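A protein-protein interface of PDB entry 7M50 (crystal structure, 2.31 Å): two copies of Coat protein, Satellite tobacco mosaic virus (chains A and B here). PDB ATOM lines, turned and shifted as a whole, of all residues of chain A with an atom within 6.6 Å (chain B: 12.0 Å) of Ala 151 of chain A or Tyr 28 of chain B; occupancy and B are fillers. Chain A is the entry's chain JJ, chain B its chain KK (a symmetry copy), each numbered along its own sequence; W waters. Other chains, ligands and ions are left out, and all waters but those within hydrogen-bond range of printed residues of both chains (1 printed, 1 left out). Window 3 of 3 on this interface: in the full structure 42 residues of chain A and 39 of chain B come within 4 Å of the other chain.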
ATOM      1  N   ILE A  41       3.892  -3.661   6.718  1.00  0.00           N
ATOM      2  CA  ILE A  41       4.737  -3.764   5.532  1.00  0.00           C
ATOM      3  C   ILE A  41       6.184  -3.517   5.946  1.00  0.00           C
ATOM      4  O   ILE A  41       6.499  -2.415   6.421  1.00  0.00           O
ATOM      5  CB  ILE A  41       4.299  -2.770   4.447  1.00  0.00           C
ATOM      6  CG1 ILE A  41       2.829  -3.000   4.085  1.00  0.00           C
ATOM      7  CG2 ILE A  41       5.186  -2.900   3.226  1.00  0.00           C
ATOM      8  CD1 ILE A  41       2.520  -4.420   3.652  1.00  0.00           C
ATOM      9  N   PRO A  42       7.081  -4.494   5.796  1.00  0.00           N
ATOM     10  CA  PRO A  42       8.498  -4.242   6.082  1.00  0.00           C
ATOM     11  C   PRO A  42       9.294  -3.898   4.832  1.00  0.00           C
ATOM     12  O   PRO A  42       9.451  -4.732   3.934  1.00  0.00           O
ATOM     13  CB  PRO A  42       8.959  -5.567   6.698  1.00  0.00           C
ATOM     14  CG  PRO A  42       8.113  -6.600   6.002  1.00  0.00           C
ATOM     15  CD  PRO A  42       6.800  -5.931   5.624  1.00  0.00           C
ATOM     16  N   PHE A  43       9.799  -2.668   4.760  1.00  0.00           N
ATOM     17  CA  PHE A  43      10.655  -2.261   3.655  1.00  0.00           C
ATOM     18  C   PHE A  43      11.710  -1.299   4.178  1.00  0.00           C
ATOM     19  O   PHE A  43      11.574  -0.727   5.263  1.00  0.00           O
ATOM     20  CB  PHE A  43       9.851  -1.626   2.511  1.00  0.00           C
ATOM     21  CG  PHE A  43       9.235  -0.300   2.856  1.00  0.00           C
ATOM     22  CD1 PHE A  43       8.028  -0.236   3.530  1.00  0.00           C
ATOM     23  CD2 PHE A  43       9.854   0.884   2.487  1.00  0.00           C
ATOM     24  CE1 PHE A  43       7.456   0.982   3.843  1.00  0.00           C
ATOM     25  CE2 PHE A  43       9.287   2.106   2.796  1.00  0.00           C
ATOM     26  CZ  PHE A  43       8.086   2.154   3.475  1.00  0.00           C
ATOM     27  N   GLU A  44      12.766  -1.127   3.389  1.00  0.00           N
ATOM     28  CA  GLU A  44      13.924  -0.341   3.785  1.00  0.00           C
ATOM     29  C   GLU A  44      14.049   0.905   2.919  1.00  0.00           C
ATOM     30  O   GLU A  44      13.683   0.905   1.740  1.00  0.00           O
ATOM     31  CB  GLU A  44      15.213  -1.164   3.683  1.00  0.00           C
ATOM     32  CG  GLU A  44      15.391  -2.190   4.789  1.00  0.00           C
ATOM     33  CD  GLU A  44      14.332  -3.271   4.758  1.00  0.00           C
ATOM     34  OE1 GLU A  44      14.092  -3.843   3.674  1.00  0.00           O
ATOM     35  OE2 GLU A  44      13.725  -3.534   5.816  1.00  0.00           O
ATOM     36  N   VAL A  45      14.578   1.968   3.520  1.00  0.00           N
ATOM     37  CA  VAL A  45      14.858   3.217   2.823  1.00  0.00           C
ATOM     38  C   VAL A  45      16.274   3.653   3.174  1.00  0.00           C
ATOM     39  O   VAL A  45      16.648   3.682   4.352  1.00  0.00           O
ATOM     40  CB  VAL A  45      13.842   4.322   3.176  1.00  0.00           C
ATOM     41  CG1 VAL A  45      12.476   3.993   2.597  1.00  0.00           C
ATOM     42  CG2 VAL A  45      13.743   4.516   4.688  1.00  0.00           C
ATOM     43  N   ARG A  79       6.838   2.577  12.395  1.00  0.00           N
ATOM     44  CA  ARG A  79       7.943   2.197  13.265  1.00  0.00           C
ATOM     45  C   ARG A  79       9.203   2.062  12.425  1.00  0.00           C
ATOM     46  O   ARG A  79       9.175   1.442  11.357  1.00  0.00           O
ATOM     47  CB  ARG A  79       7.647   0.887  13.999  1.00  0.00           C
ATOM     48  CG  ARG A  79       6.503   0.971  14.995  1.00  0.00           C
ATOM     49  CD  ARG A  79       6.302  -0.354  15.709  1.00  0.00           C
ATOM     50  NE  ARG A  79       5.919  -1.416  14.789  1.00  0.00           N
ATOM     51  CZ  ARG A  79       5.876  -2.703  15.107  1.00  0.00           C
ATOM     52  NH1 ARG A  79       6.200  -3.126  16.318  1.00  0.00           N
ATOM     53  NH2 ARG A  79       5.501  -3.586  14.187  1.00  0.00           N
ATOM     54  N   ALA A  80      10.304   2.636  12.908  1.00  0.00           N
ATOM     55  CA  ALA A  80      11.541   2.717  12.147  1.00  0.00           C
ATOM     56  C   ALA A  80      12.698   2.141  12.950  1.00  0.00           C
ATOM     57  O   ALA A  80      12.829   2.411  14.148  1.00  0.00           O
ATOM     58  CB  ALA A  80      11.856   4.166  11.757  1.00  0.00           C
ATOM     59  N   TRP A  81      13.534   1.348  12.280  1.00  0.00           N
ATOM     60  CA  TRP A  81      14.761   0.813  12.851  1.00  0.00           C
ATOM     61  C   TRP A  81      15.923   1.128  11.922  1.00  0.00           C
ATOM     62  O   TRP A  81      15.791   1.038  10.698  1.00  0.00           O
ATOM     63  CB  TRP A  81      14.680  -0.707  13.060  1.00  0.00           C
ATOM     64  CG  TRP A  81      13.747  -1.135  14.143  1.00  0.00           C
ATOM     65  CD1 TRP A  81      14.068  -1.422  15.437  1.00  0.00           C
ATOM     66  CD2 TRP A  81      12.336  -1.341  14.025  1.00  0.00           C
ATOM     67  NE1 TRP A  81      12.942  -1.787  16.135  1.00  0.00           N
ATOM     68  CE2 TRP A  81      11.865  -1.746  15.289  1.00  0.00           C
ATOM     69  CE3 TRP A  81      11.423  -1.220  12.973  1.00  0.00           C
ATOM     70  CZ2 TRP A  81      10.523  -2.028  15.531  1.00  0.00           C
ATOM     71  CZ3 TRP A  81      10.093  -1.501  13.215  1.00  0.00           C
ATOM     72  CH2 TRP A  81       9.655  -1.902  14.483  1.00  0.00           C
ATOM     73  N   THR A  82      17.059   1.501  12.507  1.00  0.00           N
ATOM     74  CA  THR A  82      18.274   1.657  11.720  1.00  0.00           C
ATOM     75  C   THR A  82      18.703   0.305  11.164  1.00  0.00           C
ATOM     76  O   THR A  82      18.659  -0.713  11.861  1.00  0.00           O
ATOM     77  CB  THR A  82      19.391   2.262  12.570  1.00  0.00           C
ATOM     78  OG1 THR A  82      19.589   1.461  13.742  1.00  0.00           O
ATOM     79  CG2 THR A  82      19.035   3.683  12.986  1.00  0.00           C
ATOM     80  N   GLN A  83      19.114   0.294   9.896  1.00  0.00           N
ATOM     81  CA  GLN A  83      19.393  -0.955   9.201  1.00  0.00           C
ATOM     82  C   GLN A  83      20.879  -1.241   9.028  1.00  0.00           C
ATOM     83  O   GLN A  83      21.246  -2.399   8.800  1.00  0.00           O
ATOM     84  CB  GLN A  83      18.704  -0.954   7.828  1.00  0.00           C
ATOM     85  CG  GLN A  83      18.728  -2.286   7.080  1.00  0.00           C
ATOM     86  CD  GLN A  83      17.863  -3.359   7.720  1.00  0.00           C
ATOM     87  OE1 GLN A  83      17.318  -3.178   8.810  1.00  0.00           O
ATOM     88  NE2 GLN A  83      17.731  -4.488   7.037  1.00  0.00           N
ATOM     89  N   ARG A 119      20.636  -1.508  17.097  1.00  0.00           N
ATOM     90  CA  ARG A 119      19.789  -0.629  16.306  1.00  0.00           C
ATOM     91  C   ARG A 119      19.229   0.506  17.161  1.00  0.00           C
ATOM     92  O   ARG A 119      19.190   0.439  18.393  1.00  0.00           O
ATOM     93  CB  ARG A 119      18.623  -1.406  15.692  1.00  0.00           C
ATOM     94  CG  ARG A 119      19.002  -2.488  14.701  1.00  0.00           C
ATOM     95  CD  ARG A 119      17.754  -3.240  14.256  1.00  0.00           C
ATOM     96  NE  ARG A 119      18.040  -4.300  13.299  1.00  0.00           N
ATOM     97  CZ  ARG A 119      17.921  -4.176  11.984  1.00  0.00           C
ATOM     98  NH1 ARG A 119      17.534  -3.039  11.429  1.00  0.00           N
ATOM     99  NH2 ARG A 119      18.195  -5.220  11.206  1.00  0.00           N
ATOM    100  N   SER A 121      15.638   2.683  17.445  1.00  0.00           N
ATOM    101  CA  SER A 121      14.243   2.502  17.074  1.00  0.00           C
ATOM    102  C   SER A 121      13.393   3.649  17.598  1.00  0.00           C
ATOM    103  O   SER A 121      13.698   4.251  18.631  1.00  0.00           O
ATOM    104  CB  SER A 121      13.694   1.172  17.607  1.00  0.00           C
ATOM    105  OG  SER A 121      13.771   1.117  19.020  1.00  0.00           O
ATOM    106  N   GLN A 149      21.072   3.367   5.950  1.00  0.00           N
ATOM    107  CA  GLN A 149      19.758   2.820   5.652  1.00  0.00           C
ATOM    108  C   GLN A 149      18.929   2.743   6.925  1.00  0.00           C
ATOM    109  O   GLN A 149      19.460   2.711   8.039  1.00  0.00           O
ATOM    110  CB  GLN A 149      19.850   1.429   5.009  1.00  0.00           C
ATOM    111  CG  GLN A 149      20.476   1.416   3.626  1.00  0.00           C
ATOM    112  CD  GLN A 149      20.359   0.062   2.952  1.00  0.00           C
ATOM    113  OE1 GLN A 149      19.573  -0.788   3.374  1.00  0.00           O
ATOM    114  NE2 GLN A 149      21.142  -0.147   1.900  1.00  0.00           N
ATOM    115  N   VAL A 150      17.610   2.718   6.744  1.00  0.00           N
ATOM    116  CA  VAL A 150      16.654   2.615   7.841  1.00  0.00           C
ATOM    117  C   VAL A 150      15.560   1.640   7.430  1.00  0.00           C
ATOM    118  O   VAL A 150      15.034   1.723   6.315  1.00  0.00           O
ATOM    119  CB  VAL A 150      16.046   3.984   8.208  1.00  0.00           C
ATOM    120  CG1 VAL A 150      14.893   3.815   9.186  1.00  0.00           C
ATOM    121  CG2 VAL A 150      17.107   4.902   8.799  1.00  0.00           C
ATOM    122  N   ALA A 151      15.224   0.713   8.323  1.00  0.00           N
ATOM    123  CA  ALA A 151      14.166  -0.258   8.085  1.00  0.00           C
ATOM    124  C   ALA A 151      12.863   0.228   8.705  1.00  0.00           C
ATOM    125  O   ALA A 151      12.851   0.749   9.824  1.00  0.00           O
ATOM    126  CB  ALA A 151      14.538  -1.626   8.658  1.00  0.00           C
ATOM    127  N   LEU A 152      11.765   0.047   7.974  1.00  0.00           N
ATOM    128  CA  LEU A 152      10.454   0.521   8.389  1.00  0.00           C
ATOM    129  C   LEU A 152       9.478  -0.642   8.495  1.00  0.00           C
ATOM    130  O   LEU A 152       9.583  -1.634   7.767  1.00  0.00           O
ATOM    131  CB  LEU A 152       9.906   1.561   7.403  1.00  0.00           C
ATOM    132  CG  LEU A 152      10.691   2.861   7.231  1.00  0.00           C
ATOM    133  CD1 LEU A 152      10.251   3.581   5.968  1.00  0.00           C
ATOM    134  CD2 LEU A 152      10.506   3.757   8.442  1.00  0.00           C
ATOM    135  N   VAL A 153       8.526  -0.511   9.418  1.00  0.00           N
ATOM    136  CA  VAL A 153       7.410  -1.442   9.556  1.00  0.00           C
ATOM    137  C   VAL A 153       6.159  -0.598   9.770  1.00  0.00           C
ATOM    138  O   VAL A 153       5.957  -0.051  10.861  1.00  0.00           O
ATOM    139  CB  VAL A 153       7.598  -2.438  10.710  1.00  0.00           C
ATOM    140  CG1 VAL A 153       6.346  -3.282  10.889  1.00  0.00           C
ATOM    141  CG2 VAL A 153       8.804  -3.331  10.455  1.00  0.00           C
ATOM    142  N   ILE B  23       5.592   6.163  19.787  1.00  0.00           N
ATOM    143  CA  ILE B  23       5.591   4.740  20.107  1.00  0.00           C
ATOM    144  C   ILE B  23       7.003   4.366  20.533  1.00  0.00           C
ATOM    145  O   ILE B  23       7.966   4.608  19.794  1.00  0.00           O
ATOM    146  CB  ILE B  23       5.130   3.888  18.915  1.00  0.00           C
ATOM    147  CG1 ILE B  23       3.718   4.287  18.486  1.00  0.00           C
ATOM    148  CG2 ILE B  23       5.187   2.406  19.267  1.00  0.00           C
ATOM    149  CD1 ILE B  23       3.204   3.514  17.290  1.00  0.00           C
ATOM    150  N   ARG B  24       7.127   3.784  21.725  1.00  0.00           N
ATOM    151  CA  ARG B  24       8.431   3.412  22.273  1.00  0.00           C
ATOM    152  C   ARG B  24       8.759   1.988  21.831  1.00  0.00           C
ATOM    153  O   ARG B  24       8.674   1.021  22.591  1.00  0.00           O
ATOM    154  CB  ARG B  24       8.434   3.562  23.789  1.00  0.00           C
ATOM    155  CG  ARG B  24       8.358   5.011  24.246  1.00  0.00           C
ATOM    156  CD  ARG B  24       8.273   5.136  25.758  1.00  0.00           C
ATOM    157  NE  ARG B  24       8.404   6.525  26.178  1.00  0.00           N
ATOM    158  CZ  ARG B  24       7.412   7.406  26.178  1.00  0.00           C
ATOM    159  NH1 ARG B  24       6.192   7.072  25.790  1.00  0.00           N
ATOM    160  NH2 ARG B  24       7.650   8.652  26.575  1.00  0.00           N
ATOM    161  N   ALA B  25       9.154   1.871  20.566  1.00  0.00           N
ATOM    162  CA  ALA B  25       9.490   0.577  19.998  1.00  0.00           C
ATOM    163  C   ALA B  25      10.795   0.054  20.589  1.00  0.00           C
ATOM    164  O   ALA B  25      11.621   0.807  21.115  1.00  0.00           O
ATOM    165  CB  ALA B  25       9.602   0.672  18.477  1.00  0.00           C
ATOM    166  N   GLY B  26      10.973  -1.260  20.496  1.00  0.00           N
ATOM    167  CA  GLY B  26      12.172  -1.897  20.999  1.00  0.00           C
ATOM    168  C   GLY B  26      13.001  -2.539  19.906  1.00  0.00           C
ATOM    169  O   GLY B  26      13.541  -1.848  19.038  1.00  0.00           O
ATOM    170  N   SER B  27      13.107  -3.864  19.938  1.00  0.00           N
ATOM    171  CA  SER B  27      13.870  -4.586  18.934  1.00  0.00           C
ATOM    172  C   SER B  27      13.052  -4.754  17.656  1.00  0.00           C
ATOM    173  O   SER B  27      11.830  -4.575  17.638  1.00  0.00           O
ATOM    174  CB  SER B  27      14.300  -5.952  19.466  1.00  0.00           C
ATOM    175  OG  SER B  27      15.080  -5.818  20.643  1.00  0.00           O
ATOM    176  N   TYR B  28      13.744  -5.097  16.578  1.00  0.00           N
ATOM    177  CA  TYR B  28      13.069  -5.326  15.306  1.00  0.00           C
ATOM    178  C   TYR B  28      12.267  -6.620  15.383  1.00  0.00           C
ATOM    179  O   TYR B  28      12.816  -7.662  15.760  1.00  0.00           O
ATOM    180  CB  TYR B  28      14.083  -5.390  14.164  1.00  0.00           C
ATOM    181  CG  TYR B  28      13.458  -5.355  12.787  1.00  0.00           C
ATOM    182  CD1 TYR B  28      13.080  -6.527  12.146  1.00  0.00           C
ATOM    183  CD2 TYR B  28      13.248  -4.152  12.127  1.00  0.00           C
ATOM    184  CE1 TYR B  28      12.505  -6.502  10.890  1.00  0.00           C
ATOM    185  CE2 TYR B  28      12.676  -4.117  10.868  1.00  0.00           C
ATOM    186  CZ  TYR B  28      12.309  -5.296  10.255  1.00  0.00           C
ATOM    187  OH  TYR B  28      11.738  -5.267   9.001  1.00  0.00           O
ATOM    188  N   PRO B  29      10.983  -6.601  15.044  1.00  0.00           N
ATOM    189  CA  PRO B  29      10.152  -7.796  15.204  1.00  0.00           C
ATOM    190  C   PRO B  29      10.284  -8.739  14.015  1.00  0.00           C
ATOM    191  O   PRO B  29      10.835  -8.401  12.967  1.00  0.00           O
ATOM    192  CB  PRO B  29       8.738  -7.218  15.290  1.00  0.00           C
ATOM    193  CG  PRO B  29       8.801  -6.015  14.404  1.00  0.00           C
ATOM    194  CD  PRO B  29      10.203  -5.453  14.547  1.00  0.00           C
ATOM    195  N   LYS B  30       9.758  -9.947  14.202  1.00  0.00           N
ATOM    196  CA  LYS B  30       9.650 -10.892  13.100  1.00  0.00           C
ATOM    197  C   LYS B  30       8.632 -10.373  12.092  1.00  0.00           C
ATOM    198  O   LYS B  30       7.512 -10.005  12.459  1.00  0.00           O
ATOM    199  CB  LYS B  30       9.238 -12.269  13.616  1.00  0.00           C
ATOM    200  CG  LYS B  30       9.993 -12.728  14.856  1.00  0.00           C
ATOM    201  CD  LYS B  30      11.492 -12.803  14.612  1.00  0.00           C
ATOM    202  CE  LYS B  30      12.234 -13.215  15.875  1.00  0.00           C
ATOM    203  NZ  LYS B  30      13.706 -13.275  15.663  1.00  0.00           N
ATOM    204  N   VAL B  31       9.023 -10.333  10.820  1.00  0.00           N
ATOM    205  CA  VAL B  31       8.201  -9.747   9.772  1.00  0.00           C
ATOM    206  C   VAL B  31       7.913 -10.803   8.710  1.00  0.00           C
ATOM    207  O   VAL B  31       8.558 -11.850   8.643  1.00  0.00           O
ATOM    208  CB  VAL B  31       8.859  -8.504   9.142  1.00  0.00           C
ATOM    209  CG1 VAL B  31       9.035  -7.410  10.186  1.00  0.00           C
ATOM    210  CG2 VAL B  31      10.196  -8.868   8.511  1.00  0.00           C
ATOM    211  N   ASN B  32       6.921 -10.508   7.874  1.00  0.00           N
ATOM    212  CA  ASN B  32       6.556 -11.367   6.756  1.00  0.00           C
ATOM    213  C   ASN B  32       5.918 -10.524   5.660  1.00  0.00           C
ATOM    214  O   ASN B  32       4.771 -10.083   5.807  1.00  0.00           O
ATOM    215  CB  ASN B  32       5.602 -12.475   7.205  1.00  0.00           C
ATOM    216  CG  ASN B  32       5.352 -13.504   6.119  1.00  0.00           C
ATOM    217  OD1 ASN B  32       6.032 -13.517   5.092  1.00  0.00           O
ATOM    218  ND2 ASN B  32       4.379 -14.380   6.344  1.00  0.00           N
ATOM    219  N   PRO B  33       6.622 -10.273   4.551  1.00  0.00           N
ATOM    220  CA  PRO B  33       6.029  -9.432   3.501  1.00  0.00           C
ATOM    221  C   PRO B  33       4.959 -10.140   2.690  1.00  0.00           C
ATOM    222  O   PRO B  33       4.074  -9.473   2.140  1.00  0.00           O
ATOM    223  CB  PRO B  33       7.239  -9.058   2.636  1.00  0.00           C
ATOM    224  CG  PRO B  33       8.158 -10.216   2.784  1.00  0.00           C
ATOM    225  CD  PRO B  33       7.989 -10.702   4.207  1.00  0.00           C
ATOM    226  N   THR B  34       5.004 -11.470   2.600  1.00  0.00           N
ATOM    227  CA  THR B  34       4.051 -12.253   1.817  1.00  0.00           C
ATOM    228  C   THR B  34       3.351 -13.234   2.750  1.00  0.00           C
ATOM    229  O   THR B  34       3.694 -14.424   2.784  1.00  0.00           O
ATOM    230  CB  THR B  34       4.746 -12.987   0.671  1.00  0.00           C
ATOM    231  OG1 THR B  34       5.772 -13.837   1.200  1.00  0.00           O
ATOM    232  CG2 THR B  34       5.369 -11.996  -0.302  1.00  0.00           C
HETATM  233  O   HOH W   1      15.011  -0.368  21.732  1.00  0.00           O
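Printed residues of chain A that touch a printed residue of chain B: Pro 42, Trp 81, Ser 121, Ala 151 and Val 153.
Of the 12 printed residues of chain B, 6 touch a printed residue of chain A.
Among the printed residues, no Asp or Glu carboxylate lies within 4 Å of a Lys or Arg side-chain nitrogen of the other chain.
Pro 42 of chain A touches just these residues of chain B: Tyr 28 (3.6 Å) and Val 31 (3.7 Å).
No residue of chain B comes within 4 Å of Glu 44 of chain A.
No residue of chain B comes within 4 Å of Val 45 of chain A.
No residue of chain B comes within 4 Å of Ala 80 of chain A.
No residue of chain B comes within 4 Å of Thr 82 of chain A.
No residue of chain B comes within 4 Å of Gln 83 of chain A.
Of the printed residues of chain B, Ser 121 of chain A touches Ala 25 and Gly 26.
No residue of chain B comes within 4 Å of Val 150 of chain A.
Ala 151 of chain A touches one residue of chain B.
Of chain B, only Tyr 28 comes within 4 Å of Val 153 of chain A.
Of the printed residues of chain A, Ala 25 of chain B touches Ser 121.
Of the printed residues of chain A, Gly 26 of chain B touches Trp 81 and Ser 121.
Printed residues of chain A within 4 Å of Ser 27 of chain B: Trp 81 (3.3 Å).
Tyr 28 of chain B touches four residues of chain A.
Printed residues of chain A within 4 Å of Val 31 of chain B: Pro 42.
The nearest residue of chain B that does not touch Ala 151 of chain A is Val 31 of chain B (8.1 Å).
O of Gly 26 of chain B lies within hydrogen-bond range of OG of Ser 121 of chain A, at 3.0 Å.
OG of Ser 121 of chain A is in hydrogen-bond range of O of Ala 25 of chain B, at 3.0 Å.
NE1 of Trp 81 of chain A lies close to O of Ser 27 of chain B (3.4 Å).
O of Gly 26 of chain B sits at hydrogen-bond distance from NE1 of Trp 81 of chain A (3.0 Å).
The indole nitrogen (NE1) of Trp 81 of chain A lies close to the backbone NH (N) of Tyr 28 of chain B (3.4 Å).
No position is printed for both chains.
Of the 10 pairs that touch across the chains among the printed residues, none has its exchanged pair printed and touching as well.
Water W1 lies within hydrogen-bond range of OG of Ser 121 of chain A (3.3 Å) and O of Gly 26 of chain B (3.4 Å).
The backbone carbonyl oxygen of Trp 81 of chain A lies within hydrogen-bond range of the backbone NH of Ala 151 of chain A.
The backbone carbonyl oxygen (O) of Arg 79 of chain A is in hydrogen-bond range of the backbone NH (N) of Val 153 of chain A (2.8 Å).
Pro 42 of chain A touches Tyr 28 of chain B.
Pro 42 of chain A touches Val 31 of chain B.
Trp 81 of chain A touches Pro 29 of chain B.
CE2 of Tyr 28 of chain B touches CB of Ala 151 of chain A, at 3.8 Å.
CG2 of Val 153 of chain A touches OH of Tyr 28 of chain B, at 3.8 Å.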
